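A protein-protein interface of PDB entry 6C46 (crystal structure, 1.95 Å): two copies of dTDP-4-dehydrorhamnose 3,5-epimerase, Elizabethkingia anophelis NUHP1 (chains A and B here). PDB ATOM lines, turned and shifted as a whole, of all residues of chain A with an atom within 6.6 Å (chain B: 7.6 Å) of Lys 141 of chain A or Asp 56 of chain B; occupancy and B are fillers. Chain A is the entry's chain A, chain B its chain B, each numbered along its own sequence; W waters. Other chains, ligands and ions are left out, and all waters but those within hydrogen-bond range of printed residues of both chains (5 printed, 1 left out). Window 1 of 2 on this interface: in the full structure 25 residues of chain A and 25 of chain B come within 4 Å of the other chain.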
ATOM      1  N   TYR A  35      33.871   3.033  12.725  1.00  0.00           N
ATOM      2  CA  TYR A  35      33.661   3.043  14.165  1.00  0.00           C
ATOM      3  C   TYR A  35      33.231   1.666  14.633  1.00  0.00           C
ATOM      4  O   TYR A  35      32.697   0.858  13.860  1.00  0.00           O
ATOM      5  CB  TYR A  35      32.635   4.096  14.625  1.00  0.00           C
ATOM      6  CG  TYR A  35      31.201   3.957  14.138  1.00  0.00           C
ATOM      7  CD1 TYR A  35      30.214   3.470  14.989  1.00  0.00           C
ATOM      8  CD2 TYR A  35      30.814   4.405  12.863  1.00  0.00           C
ATOM      9  CE1 TYR A  35      28.874   3.390  14.577  1.00  0.00           C
ATOM     10  CE2 TYR A  35      29.467   4.330  12.443  1.00  0.00           C
ATOM     11  CZ  TYR A  35      28.520   3.809  13.301  1.00  0.00           C
ATOM     12  OH  TYR A  35      27.201   3.734  12.908  1.00  0.00           O
ATOM     13  N   GLU A  36      33.525   1.404  15.904  1.00  0.00           N
ATOM     14  CA  GLU A  36      33.039   0.227  16.606  1.00  0.00           C
ATOM     15  C   GLU A  36      31.643   0.553  17.113  1.00  0.00           C
ATOM     16  O   GLU A  36      31.476   1.365  18.021  1.00  0.00           O
ATOM     17  CB  GLU A  36      33.976  -0.150  17.756  1.00  0.00           C
ATOM     18  CG  GLU A  36      33.537  -1.422  18.512  1.00  0.00           C
ATOM     19  CD  GLU A  36      34.433  -1.736  19.703  1.00  0.00           C
ATOM     20  OE1 GLU A  36      34.477  -0.932  20.661  1.00  0.00           O
ATOM     21  OE2 GLU A  36      35.097  -2.791  19.666  1.00  0.00           O
ATOM     22  N   LYS A  37      30.630  -0.051  16.506  1.00  0.00           N
ATOM     23  CA  LYS A  37      29.269   0.271  16.891  1.00  0.00           C
ATOM     24  C   LYS A  37      28.923  -0.315  18.250  1.00  0.00           C
ATOM     25  O   LYS A  37      28.284   0.346  19.065  1.00  0.00           O
ATOM     26  CB  LYS A  37      28.305  -0.264  15.833  1.00  0.00           C
ATOM     27  CG  LYS A  37      26.855   0.046  16.118  1.00  0.00           C
ATOM     28  CD  LYS A  37      26.024  -0.174  14.814  1.00  0.00           C
ATOM     29  CE  LYS A  37      24.518  -0.043  15.093  1.00  0.00           C
ATOM     30  NZ  LYS A  37      23.693  -0.032  13.833  1.00  0.00           N
ATOM     31  N   TYR A  38      29.329  -1.557  18.510  1.00  0.00           N
ATOM     32  CA  TYR A  38      28.938  -2.200  19.758  1.00  0.00           C
ATOM     33  C   TYR A  38      30.014  -3.202  20.126  1.00  0.00           C
ATOM     34  O   TYR A  38      30.626  -3.820  19.251  1.00  0.00           O
ATOM     35  CB  TYR A  38      27.573  -2.915  19.637  1.00  0.00           C
ATOM     36  CG  TYR A  38      27.218  -3.667  20.904  1.00  0.00           C
ATOM     37  CD1 TYR A  38      26.858  -2.978  22.057  1.00  0.00           C
ATOM     38  CD2 TYR A  38      27.292  -5.059  20.957  1.00  0.00           C
ATOM     39  CE1 TYR A  38      26.555  -3.645  23.224  1.00  0.00           C
ATOM     40  CE2 TYR A  38      26.988  -5.748  22.144  1.00  0.00           C
ATOM     41  CZ  TYR A  38      26.617  -5.018  23.266  1.00  0.00           C
ATOM     42  OH  TYR A  38      26.312  -5.643  24.456  1.00  0.00           O
ATOM     43  N   ASN A  39      30.216  -3.377  21.429  1.00  0.00           N
ATOM     44  CA  ASN A  39      31.215  -4.320  21.925  1.00  0.00           C
ATOM     45  C   ASN A  39      30.663  -4.898  23.223  1.00  0.00           C
ATOM     46  O   ASN A  39      30.463  -4.158  24.180  1.00  0.00           O
ATOM     47  CB  ASN A  39      32.575  -3.617  22.134  1.00  0.00           C
ATOM     48  CG  ASN A  39      33.641  -4.549  22.695  1.00  0.00           C
ATOM     49  OD1 ASN A  39      33.398  -5.234  23.688  1.00  0.00           O
ATOM     50  ND2 ASN A  39      34.839  -4.580  22.061  1.00  0.00           N
ATOM     51  N   GLU A  40      30.409  -6.202  23.252  1.00  0.00           N
ATOM     52  CA  GLU A  40      29.738  -6.800  24.400  1.00  0.00           C
ATOM     53  C   GLU A  40      30.577  -6.685  25.671  1.00  0.00           C
ATOM     54  O   GLU A  40      30.043  -6.415  26.750  1.00  0.00           O
ATOM     55  CB  GLU A  40      29.415  -8.264  24.090  1.00  0.00           C
ATOM     56  CG  GLU A  40      28.821  -8.997  25.298  1.00  0.00           C
ATOM     57  CD  GLU A  40      28.364 -10.400  24.945  1.00  0.00           C
ATOM     58  OE1 GLU A  40      27.969 -10.633  23.770  1.00  0.00           O
ATOM     59  OE2 GLU A  40      28.336 -11.249  25.855  1.00  0.00           O
ATOM     60  N   PHE A  53      23.425 -10.148  22.758  1.00  0.00           N
ATOM     61  CA  PHE A  53      22.260 -10.079  21.878  1.00  0.00           C
ATOM     62  C   PHE A  53      22.189 -11.306  20.975  1.00  0.00           C
ATOM     63  O   PHE A  53      23.219 -11.785  20.492  1.00  0.00           O
ATOM     64  CB  PHE A  53      22.300  -8.785  21.066  1.00  0.00           C
ATOM     65  CG  PHE A  53      22.122  -7.569  21.953  1.00  0.00           C
ATOM     66  CD1 PHE A  53      20.858  -7.130  22.306  1.00  0.00           C
ATOM     67  CD2 PHE A  53      23.226  -6.958  22.526  1.00  0.00           C
ATOM     68  CE1 PHE A  53      20.689  -6.044  23.179  1.00  0.00           C
ATOM     69  CE2 PHE A  53      23.078  -5.867  23.401  1.00  0.00           C
ATOM     70  CZ  PHE A  53      21.800  -5.409  23.719  1.00  0.00           C
ATOM     71  N   VAL A  54      20.969 -11.819  20.773  1.00  0.00           N
ATOM     72  CA  VAL A  54      20.745 -13.107  20.121  1.00  0.00           C
ATOM     73  C   VAL A  54      19.906 -12.997  18.856  1.00  0.00           C
ATOM     74  O   VAL A  54      19.740 -14.004  18.143  1.00  0.00           O
ATOM     75  CB  VAL A  54      20.066 -14.115  21.080  1.00  0.00           C
ATOM     76  CG1 VAL A  54      20.938 -14.389  22.303  1.00  0.00           C
ATOM     77  CG2 VAL A  54      18.686 -13.608  21.488  1.00  0.00           C
ATOM     78  N   GLN A  55      19.330 -11.838  18.574  1.00  0.00           N
ATOM     79  CA  GLN A  55      18.436 -11.694  17.446  1.00  0.00           C
ATOM     80  C   GLN A  55      18.561 -10.264  16.942  1.00  0.00           C
ATOM     81  O   GLN A  55      18.677  -9.331  17.742  1.00  0.00           O
ATOM     82  CB  GLN A  55      16.993 -11.970  17.852  1.00  0.00           C
ATOM     83  CG  GLN A  55      16.028 -11.705  16.748  1.00  0.00           C
ATOM     84  CD  GLN A  55      14.608 -11.638  17.231  1.00  0.00           C
ATOM     85  OE1 GLN A  55      14.232 -10.710  17.949  1.00  0.00           O
ATOM     86  NE2 GLN A  55      13.802 -12.613  16.836  1.00  0.00           N
ATOM     87  N   ASP A  56      18.559 -10.097  15.629  1.00  0.00           N
ATOM     88  CA  ASP A  56      18.584  -8.781  14.993  1.00  0.00           C
ATOM     89  C   ASP A  56      17.398  -8.681  14.052  1.00  0.00           C
ATOM     90  O   ASP A  56      17.177  -9.591  13.247  1.00  0.00           O
ATOM     91  CB  ASP A  56      19.877  -8.562  14.192  1.00  0.00           C
ATOM     92  CG  ASP A  56      21.127  -8.759  15.029  1.00  0.00           C
ATOM     93  OD1 ASP A  56      21.009  -8.850  16.269  1.00  0.00           O
ATOM     94  OD2 ASP A  56      22.230  -8.833  14.448  1.00  0.00           O
ATOM     95  N   ASN A  57      16.663  -7.564  14.127  1.00  0.00           N
ATOM     96  CA  ASN A  57      15.458  -7.360  13.334  1.00  0.00           C
ATOM     97  C   ASN A  57      15.564  -6.032  12.602  1.00  0.00           C
ATOM     98  O   ASN A  57      16.146  -5.072  13.113  1.00  0.00           O
ATOM     99  CB  ASN A  57      14.204  -7.344  14.223  1.00  0.00           C
ATOM    100  CG  ASN A  57      14.148  -8.535  15.160  1.00  0.00           C
ATOM    101  OD1 ASN A  57      13.779  -9.618  14.745  1.00  0.00           O
ATOM    102  ND2 ASN A  57      14.512  -8.331  16.435  1.00  0.00           N
ATOM    103  N   ALA A  79      15.627  -7.154  26.329  1.00  0.00           N
ATOM    104  CA  ALA A  79      16.357  -5.900  26.207  1.00  0.00           C
ATOM    105  C   ALA A  79      16.580  -5.616  24.730  1.00  0.00           C
ATOM    106  O   ALA A  79      16.775  -6.546  23.940  1.00  0.00           O
ATOM    107  CB  ALA A  79      17.704  -5.968  26.948  1.00  0.00           C
ATOM    108  N   LYS A  80      16.534  -4.328  24.351  1.00  0.00           N
ATOM    109  CA  LYS A  80      16.602  -3.911  22.956  1.00  0.00           C
ATOM    110  C   LYS A  80      17.687  -2.860  22.781  1.00  0.00           C
ATOM    111  O   LYS A  80      17.762  -1.912  23.564  1.00  0.00           O
ATOM    112  CB  LYS A  80      15.252  -3.365  22.476  1.00  0.00           C
ATOM    113  CG  LYS A  80      14.144  -4.436  22.498  1.00  0.00           C
ATOM    114  CD  LYS A  80      12.731  -3.842  22.432  1.00  0.00           C
ATOM    115  CE  LYS A  80      11.656  -4.936  22.581  1.00  0.00           C
ATOM    116  NZ  LYS A  80      10.265  -4.360  22.845  1.00  0.00           N
ATOM    117  N   LEU A  81      18.527  -3.034  21.761  1.00  0.00           N
ATOM    118  CA  LEU A  81      19.520  -2.038  21.364  1.00  0.00           C
ATOM    119  C   LEU A  81      19.099  -1.559  19.990  1.00  0.00           C
ATOM    120  O   LEU A  81      19.162  -2.323  19.022  1.00  0.00           O
ATOM    121  CB  LEU A  81      20.923  -2.637  21.326  1.00  0.00           C
ATOM    122  CG  LEU A  81      22.051  -1.656  21.019  1.00  0.00           C
ATOM    123  CD1 LEU A  81      22.153  -0.567  22.084  1.00  0.00           C
ATOM    124  CD2 LEU A  81      23.343  -2.466  20.926  1.00  0.00           C
ATOM    125  N   VAL A  82      18.642  -0.318  19.901  1.00  0.00           N
ATOM    126  CA  VAL A  82      17.947   0.115  18.702  1.00  0.00           C
ATOM    127  C   VAL A  82      18.689   1.272  18.057  1.00  0.00           C
ATOM    128  O   VAL A  82      19.368   2.062  18.723  1.00  0.00           O
ATOM    129  CB  VAL A  82      16.477   0.488  19.022  1.00  0.00           C
ATOM    130  CG1 VAL A  82      15.763  -0.670  19.701  1.00  0.00           C
ATOM    131  CG2 VAL A  82      16.410   1.669  19.953  1.00  0.00           C
ATOM    132  N   SER A  83      18.572   1.358  16.734  1.00  0.00           N
ATOM    133  CA  SER A  83      19.171   2.466  16.002  1.00  0.00           C
ATOM    134  C   SER A  83      18.443   2.610  14.682  1.00  0.00           C
ATOM    135  O   SER A  83      17.623   1.777  14.301  1.00  0.00           O
ATOM    136  CB  SER A  83      20.677   2.262  15.783  1.00  0.00           C
ATOM    137  OG  SER A  83      20.934   1.054  15.060  1.00  0.00           O
ATOM    138  N   GLN A 118      22.731   4.867  19.247  1.00  0.00           N
ATOM    139  CA  GLN A 118      21.973   3.689  19.633  1.00  0.00           C
ATOM    140  C   GLN A 118      21.362   3.924  21.006  1.00  0.00           C
ATOM    141  O   GLN A 118      21.929   4.631  21.842  1.00  0.00           O
ATOM    142  CB  GLN A 118      22.849   2.453  19.705  1.00  0.00           C
ATOM    143  CG  GLN A 118      23.544   2.108  18.393  1.00  0.00           C
ATOM    144  CD  GLN A 118      24.647   1.131  18.680  1.00  0.00           C
ATOM    145  OE1 GLN A 118      24.418  -0.067  18.683  1.00  0.00           O
ATOM    146  NE2 GLN A 118      25.841   1.648  19.002  1.00  0.00           N
ATOM    147  N   SER A 139      16.538  -0.568  13.142  1.00  0.00           N
ATOM    148  CA  SER A 139      17.243  -1.791  13.518  1.00  0.00           C
ATOM    149  C   SER A 139      17.058  -2.022  15.009  1.00  0.00           C
ATOM    150  O   SER A 139      17.258  -1.104  15.813  1.00  0.00           O
ATOM    151  CB  SER A 139      18.733  -1.675  13.173  1.00  0.00           C
ATOM    152  OG  SER A 139      19.523  -2.520  13.990  1.00  0.00           O
ATOM    153  N   TYR A 140      16.660  -3.230  15.394  1.00  0.00           N
ATOM    154  CA  TYR A 140      16.643  -3.520  16.822  1.00  0.00           C
ATOM    155  C   TYR A 140      17.203  -4.908  17.079  1.00  0.00           C
ATOM    156  O   TYR A 140      16.798  -5.880  16.438  1.00  0.00           O
ATOM    157  CB  TYR A 140      15.250  -3.347  17.446  1.00  0.00           C
ATOM    158  CG  TYR A 140      14.074  -4.105  16.888  1.00  0.00           C
ATOM    159  CD1 TYR A 140      13.491  -5.137  17.624  1.00  0.00           C
ATOM    160  CD2 TYR A 140      13.491  -3.753  15.673  1.00  0.00           C
ATOM    161  CE1 TYR A 140      12.397  -5.825  17.157  1.00  0.00           C
ATOM    162  CE2 TYR A 140      12.397  -4.432  15.194  1.00  0.00           C
ATOM    163  CZ  TYR A 140      11.851  -5.470  15.941  1.00  0.00           C
ATOM    164  OH  TYR A 140      10.758  -6.155  15.472  1.00  0.00           O
ATOM    165  N   LYS A 141      18.183  -4.964  17.971  1.00  0.00           N
ATOM    166  CA  LYS A 141      18.777  -6.198  18.461  1.00  0.00           C
ATOM    167  C   LYS A 141      18.139  -6.517  19.800  1.00  0.00           C
ATOM    168  O   LYS A 141      17.962  -5.622  20.637  1.00  0.00           O
ATOM    169  CB  LYS A 141      20.290  -6.052  18.637  1.00  0.00           C
ATOM    170  CG  LYS A 141      21.024  -5.380  17.458  1.00  0.00           C
ATOM    171  CD  LYS A 141      22.557  -5.509  17.572  1.00  0.00           C
ATOM    172  CE  LYS A 141      23.048  -6.960  17.430  1.00  0.00           C
ATOM    173  NZ  LYS A 141      24.536  -7.150  17.479  1.00  0.00           N
ATOM    174  N   CYS A 142      17.815  -7.787  20.016  1.00  0.00           N
ATOM    175  CA  CYS A 142      17.141  -8.204  21.238  1.00  0.00           C
ATOM    176  C   CYS A 142      18.014  -9.193  21.973  1.00  0.00           C
ATOM    177  O   CYS A 142      18.623 -10.061  21.344  1.00  0.00           O
ATOM    178  CB  CYS A 142      15.808  -8.859  20.950  1.00  0.00           C
ATOM    179  SG  CYS A 142      14.671  -7.775  20.063  1.00  0.00           S
ATOM    180  N   ASP A 143      18.012  -9.102  23.308  1.00  0.00           N
ATOM    181  CA  ASP A 143      18.773 -10.030  24.133  1.00  0.00           C
ATOM    182  C   ASP A 143      17.940 -11.237  24.567  1.00  0.00           C
ATOM    183  O   ASP A 143      18.349 -11.978  25.463  1.00  0.00           O
ATOM    184  CB  ASP A 143      19.415  -9.276  25.320  1.00  0.00           C
ATOM    185  CG  ASP A 143      18.520  -9.185  26.561  1.00  0.00           C
ATOM    186  OD1 ASP A 143      17.283  -9.342  26.498  1.00  0.00           O
ATOM    187  OD2 ASP A 143      19.090  -8.914  27.642  1.00  0.00           O
ATOM    188  N   ASN A 144      16.810 -11.490  23.898  1.00  0.00           N
ATOM    189  CA  ASN A 144      16.004 -12.668  24.179  1.00  0.00           C
ATOM    190  C   ASN A 144      15.175 -12.949  22.941  1.00  0.00           C
ATOM    191  O   ASN A 144      14.989 -12.074  22.089  1.00  0.00           O
ATOM    192  CB  ASN A 144      15.115 -12.440  25.417  1.00  0.00           C
ATOM    193  CG  ASN A 144      14.777 -13.712  26.163  1.00  0.00           C
ATOM    194  OD1 ASN A 144      14.946 -14.835  25.663  1.00  0.00           O
ATOM    195  ND2 ASN A 144      14.256 -13.541  27.380  1.00  0.00           N
ATOM    196  N   TYR B  38      18.907 -11.795  11.790  1.00  0.00           N
ATOM    197  CA  TYR B  38      19.788 -12.814  12.340  1.00  0.00           C
ATOM    198  C   TYR B  38      19.149 -13.388  13.594  1.00  0.00           C
ATOM    199  O   TYR B  38      18.473 -12.679  14.340  1.00  0.00           O
ATOM    200  CB  TYR B  38      21.172 -12.244  12.691  1.00  0.00           C
ATOM    201  CG  TYR B  38      22.083 -13.273  13.317  1.00  0.00           C
ATOM    202  CD1 TYR B  38      22.626 -14.301  12.548  1.00  0.00           C
ATOM    203  CD2 TYR B  38      22.377 -13.236  14.673  1.00  0.00           C
ATOM    204  CE1 TYR B  38      23.452 -15.283  13.120  1.00  0.00           C
ATOM    205  CE2 TYR B  38      23.203 -14.208  15.265  1.00  0.00           C
ATOM    206  CZ  TYR B  38      23.747 -15.216  14.481  1.00  0.00           C
ATOM    207  OH  TYR B  38      24.539 -16.183  15.079  1.00  0.00           O
ATOM    208  N   PHE B  53      27.891 -13.467  18.473  1.00  0.00           N
ATOM    209  CA  PHE B  53      28.727 -12.360  18.020  1.00  0.00           C
ATOM    210  C   PHE B  53      28.868 -11.332  19.131  1.00  0.00           C
ATOM    211  O   PHE B  53      27.901 -11.062  19.851  1.00  0.00           O
ATOM    212  CB  PHE B  53      28.126 -11.739  16.763  1.00  0.00           C
ATOM    213  CG  PHE B  53      28.222 -12.661  15.581  1.00  0.00           C
ATOM    214  CD1 PHE B  53      27.215 -13.573  15.309  1.00  0.00           C
ATOM    215  CD2 PHE B  53      29.372 -12.680  14.801  1.00  0.00           C
ATOM    216  CE1 PHE B  53      27.325 -14.482  14.251  1.00  0.00           C
ATOM    217  CE2 PHE B  53      29.495 -13.593  13.742  1.00  0.00           C
ATOM    218  CZ  PHE B  53      28.466 -14.480  13.465  1.00  0.00           C
ATOM    219  N   VAL B  54      30.074 -10.766  19.265  1.00  0.00           N
ATOM    220  CA  VAL B  54      30.439  -9.933  20.413  1.00  0.00           C
ATOM    221  C   VAL B  54      30.812  -8.510  20.032  1.00  0.00           C
ATOM    222  O   VAL B  54      30.941  -7.654  20.935  1.00  0.00           O
ATOM    223  CB  VAL B  54      31.598 -10.553  21.223  1.00  0.00           C
ATOM    224  CG1 VAL B  54      31.176 -11.898  21.858  1.00  0.00           C
ATOM    225  CG2 VAL B  54      32.822 -10.699  20.335  1.00  0.00           C
ATOM    226  N   GLN B  55      30.954  -8.210  18.746  1.00  0.00           N
ATOM    227  CA  GLN B  55      31.433  -6.900  18.326  1.00  0.00           C
ATOM    228  C   GLN B  55      30.781  -6.588  16.988  1.00  0.00           C
ATOM    229  O   GLN B  55      30.687  -7.459  16.131  1.00  0.00           O
ATOM    230  CB  GLN B  55      32.966  -6.889  18.199  1.00  0.00           C
ATOM    231  CG  GLN B  55      33.523  -5.615  17.641  1.00  0.00           C
ATOM    232  CD  GLN B  55      34.980  -5.728  17.264  1.00  0.00           C
ATOM    233  OE1 GLN B  55      35.337  -6.455  16.341  1.00  0.00           O
ATOM    234  NE2 GLN B  55      35.823  -4.972  17.943  1.00  0.00           N
ATOM    235  N   ASP B  56      30.301  -5.366  16.827  1.00  0.00           N
ATOM    236  CA  ASP B  56      29.738  -4.905  15.568  1.00  0.00           C
ATOM    237  C   ASP B  56      30.523  -3.679  15.144  1.00  0.00           C
ATOM    238  O   ASP B  56      30.739  -2.769  15.954  1.00  0.00           O
ATOM    239  CB  ASP B  56      28.248  -4.535  15.678  1.00  0.00           C
ATOM    240  CG  ASP B  56      27.376  -5.687  16.143  1.00  0.00           C
ATOM    241  OD1 ASP B  56      27.734  -6.861  15.912  1.00  0.00           O
ATOM    242  OD2 ASP B  56      26.313  -5.411  16.739  1.00  0.00           O
ATOM    243  N   ASN B  57      30.915  -3.645  13.872  1.00  0.00           N
ATOM    244  CA  ASN B  57      31.750  -2.590  13.320  1.00  0.00           C
ATOM    245  C   ASN B  57      31.094  -2.042  12.068  1.00  0.00           C
ATOM    246  O   ASN B  57      30.444  -2.784  11.323  1.00  0.00           O
ATOM    247  CB  ASN B  57      33.138  -3.127  12.962  1.00  0.00           C
ATOM    248  CG  ASN B  57      33.770  -3.859  14.121  1.00  0.00           C
ATOM    249  OD1 ASN B  57      34.307  -3.237  15.026  1.00  0.00           O
ATOM    250  ND2 ASN B  57      33.680  -5.186  14.111  1.00  0.00           N
ATOM    251  N   ILE B  58      31.294  -0.753  11.837  1.00  0.00           N
ATOM    252  CA  ILE B  58      30.732  -0.046  10.691  1.00  0.00           C
ATOM    253  C   ILE B  58      31.857   0.712  10.002  1.00  0.00           C
ATOM    254  O   ILE B  58      32.699   1.328  10.667  1.00  0.00           O
ATOM    255  CB  ILE B  58      29.626   0.935  11.132  1.00  0.00           C
ATOM    256  CG1 ILE B  58      28.483   0.189  11.839  1.00  0.00           C
ATOM    257  CG2 ILE B  58      29.134   1.774   9.952  1.00  0.00           C
ATOM    258  CD1 ILE B  58      27.634  -0.689  10.927  1.00  0.00           C
ATOM    259  N   LEU B  81      30.207 -11.919  10.180  1.00  0.00           N
ATOM    260  CA  LEU B  81      28.916 -11.914   9.521  1.00  0.00           C
ATOM    261  C   LEU B  81      28.772 -10.533   8.908  1.00  0.00           C
ATOM    262  O   LEU B  81      28.632  -9.547   9.637  1.00  0.00           O
ATOM    263  CB  LEU B  81      27.797 -12.228  10.502  1.00  0.00           C
ATOM    264  CG  LEU B  81      26.432 -12.281   9.807  1.00  0.00           C
ATOM    265  CD1 LEU B  81      26.405 -13.373   8.732  1.00  0.00           C
ATOM    266  CD2 LEU B  81      25.305 -12.485  10.837  1.00  0.00           C
ATOM    267  N   SER B 139      28.892  -3.331   7.130  1.00  0.00           N
ATOM    268  CA  SER B 139      28.653  -3.749   8.505  1.00  0.00           C
ATOM    269  C   SER B 139      29.333  -5.091   8.720  1.00  0.00           C
ATOM    270  O   SER B 139      29.198  -6.000   7.886  1.00  0.00           O
ATOM    271  CB  SER B 139      27.148  -3.891   8.788  1.00  0.00           C
ATOM    272  OG  SER B 139      26.912  -4.764   9.880  1.00  0.00           O
ATOM    273  N   TYR B 140      30.109  -5.222   9.792  1.00  0.00           N
ATOM    274  CA  TYR B 140      30.599  -6.561  10.076  1.00  0.00           C
ATOM    275  C   TYR B 140      30.552  -6.859  11.560  1.00  0.00           C
ATOM    276  O   TYR B 140      31.079  -6.098  12.379  1.00  0.00           O
ATOM    277  CB  TYR B 140      32.002  -6.809   9.486  1.00  0.00           C
ATOM    278  CG  TYR B 140      33.115  -5.868   9.819  1.00  0.00           C
ATOM    279  CD1 TYR B 140      34.145  -6.265  10.662  1.00  0.00           C
ATOM    280  CD2 TYR B 140      33.178  -4.609   9.250  1.00  0.00           C
ATOM    281  CE1 TYR B 140      35.193  -5.418  10.957  1.00  0.00           C
ATOM    282  CE2 TYR B 140      34.223  -3.756   9.528  1.00  0.00           C
ATOM    283  CZ  TYR B 140      35.227  -4.166  10.386  1.00  0.00           C
ATOM    284  OH  TYR B 140      36.263  -3.312  10.671  1.00  0.00           O
ATOM    285  N   LYS B 141      29.912  -7.976  11.886  1.00  0.00           N
ATOM    286  CA  LYS B 141      29.869  -8.495  13.243  1.00  0.00           C
ATOM    287  C   LYS B 141      30.943  -9.554  13.371  1.00  0.00           C
ATOM    288  O   LYS B 141      31.123 -10.372  12.464  1.00  0.00           O
ATOM    289  CB  LYS B 141      28.501  -9.104  13.569  1.00  0.00           C
ATOM    290  CG  LYS B 141      27.341  -8.237  13.096  1.00  0.00           C
ATOM    291  CD  LYS B 141      26.037  -8.576  13.782  1.00  0.00           C
ATOM    292  CE  LYS B 141      25.651 -10.020  13.635  1.00  0.00           C
ATOM    293  NZ  LYS B 141      24.753 -10.405  14.766  1.00  0.00           N
ATOM    294  N   CYS B 142      31.645  -9.542  14.493  1.00  0.00           N
ATOM    295  CA  CYS B 142      32.735 -10.472  14.738  1.00  0.00           C
ATOM    296  C   CYS B 142      32.407 -11.313  15.949  1.00  0.00           C
ATOM    297  O   CYS B 142      31.857 -10.797  16.927  1.00  0.00           O
ATOM    298  CB  CYS B 142      34.057  -9.733  14.978  1.00  0.00           C
ATOM    299  SG  CYS B 142      34.544  -8.711  13.549  1.00  0.00           S
HETATM  300  O   HOH W   1      26.184  -9.698  21.755  1.00  0.00           O
HETATM  301  O   HOH W   2      23.170 -10.326  17.426  1.00  0.00           O
HETATM  302  O   HOH W   3      24.758 -13.247  18.651  1.00  0.00           O
HETATM  303  O   HOH W   4      35.111  -0.176  11.674  1.00  0.00           O
HETATM  304  O   HOH W   5      37.405  -6.012  20.262  1.00  0.00           O
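Printed residues of chain A that touch a printed residue of chain B: Tyr 35, Glu 36, Lys 37, Tyr 38, Asn 39, Glu 40, Gln 55, Asp 56 and Lys 141.
Hydrophobic or aromatic side chains of chain A within 4 Å of the printed part of chain B: Tyr 35.
Among the printed residues, 15 pairs touch across the chains.
Water W1 lies within hydrogen-bond range of the side-chain carboxylate (OE1) of Glu 40 of chain A, the backbone carbonyl oxygen (O) of Phe 53 of chain B and the backbone NH (N) of Phe 53 of chain A.
Water W2 lies within hydrogen-bond range of OD1 of Asp 56 of chain A, NZ of Lys 141 of chain B, O of Phe 53 of chain A and NZ of Lys 141 of chain A.
Water W5 lies within hydrogen-bond range of the side-chain amide nitrogen of Gln 55 of chain B and the side-chain amide nitrogen of Asn 39 of chain A.
Tyr 38 of chain A touches Gln 55 of chain B, and with the chains exchanged Gln 55 of chain A touches Tyr 38 of chain B.
Tyr 38 of chain A touches Asp 56 of chain B, and with the chains exchanged Asp 56 of chain A touches Tyr 38 of chain B.
Asp 56 of chain A touches Lys 141 of chain B, and with the chains exchanged Lys 141 of chain A touches Asp 56 of chain B.
The side-chain amide oxygen (OE1) of Gln 55 of chain B is in hydrogen-bond range of the side-chain amide nitrogen (ND2) of Asn 57 of chain B, at 3.1 Å.
O of Gln 55 of chain B is in hydrogen-bond range of N of Cys 142 of chain B (2.8 Å).
The side-chain sulfur (SG) of Cys 142 of chain B is in hydrogen-bond range of the side-chain amide nitrogen (ND2) of Asn 57 of chain B.
N of Tyr 35 of chain A is in hydrogen-bond range of O of Ile 58 of chain B, at 2.9 Å.
The side-chain carboxylate (OE2) of Glu 36 of chain A sits at hydrogen-bond distance from the side-chain amide nitrogen (NE2) of Gln 55 of chain B (2.9 Å).
The backbone NH (N) of Lys 37 of chain A lies within hydrogen-bond range of the backbone carbonyl oxygen (O) of Asp 56 of chain B (2.8 Å).
O of Tyr 38 of chain A lies within hydrogen-bond range of N of Asp 56 of chain B (2.9 Å).
The backbone NH (N) of Glu 40 of chain A sits at hydrogen-bond distance from the backbone carbonyl oxygen (O) of Val 54 of chain B.
The backbone carbonyl oxygen (O) of Tyr 38 of chain B sits at hydrogen-bond distance from the backbone NH (N) of Asp 56 of chain A, at 2.9 Å.
The side-chain amino group (NZ) of Lys 141 of chain B lies within salt-bridge range of the side-chain carboxylate (OD2) of Asp 56 of chain A (3.0 Å).
NZ of Lys 141 of chain A is in salt-bridge range of OD2 of Asp 56 of chain B (2.6 Å).
Lys 141 of chain A touches just one residue of chain B: Asp 56.
Of the printed residues of chain A, Asp 56 of chain B touches Glu 36 (3.6 Å), Lys 37 (2.8 Å), Tyr 38 (2.9 Å) and Lys 141 (2.6 Å).
Printed residues of chain B within 4 Å of Gln 55 of chain A: Tyr 38 (3.3 Å).
Of the printed residues of chain B, Tyr 38 of chain A touches Gln 55 and Asp 56.
The nearest residue of chain B that does not touch Lys 141 of chain A is Lys 141 of chain B (4.2 Å).
Among the printed residues, pairs that only touch across the chains: Tyr 35 of chain A with Asn 57 of chain B, Glu 36 of chain A with Asp 56 of chain B, Lys 37 of chain A with Ile 58 of chain B, Tyr 38 of chain A with Gln 55 of chain B, Asn 39 of chain A with Val 54 of chain B, Glu 40 of chain A with Phe 53 of chain B and Gln 55 of chain A with Tyr 38 of chain B.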
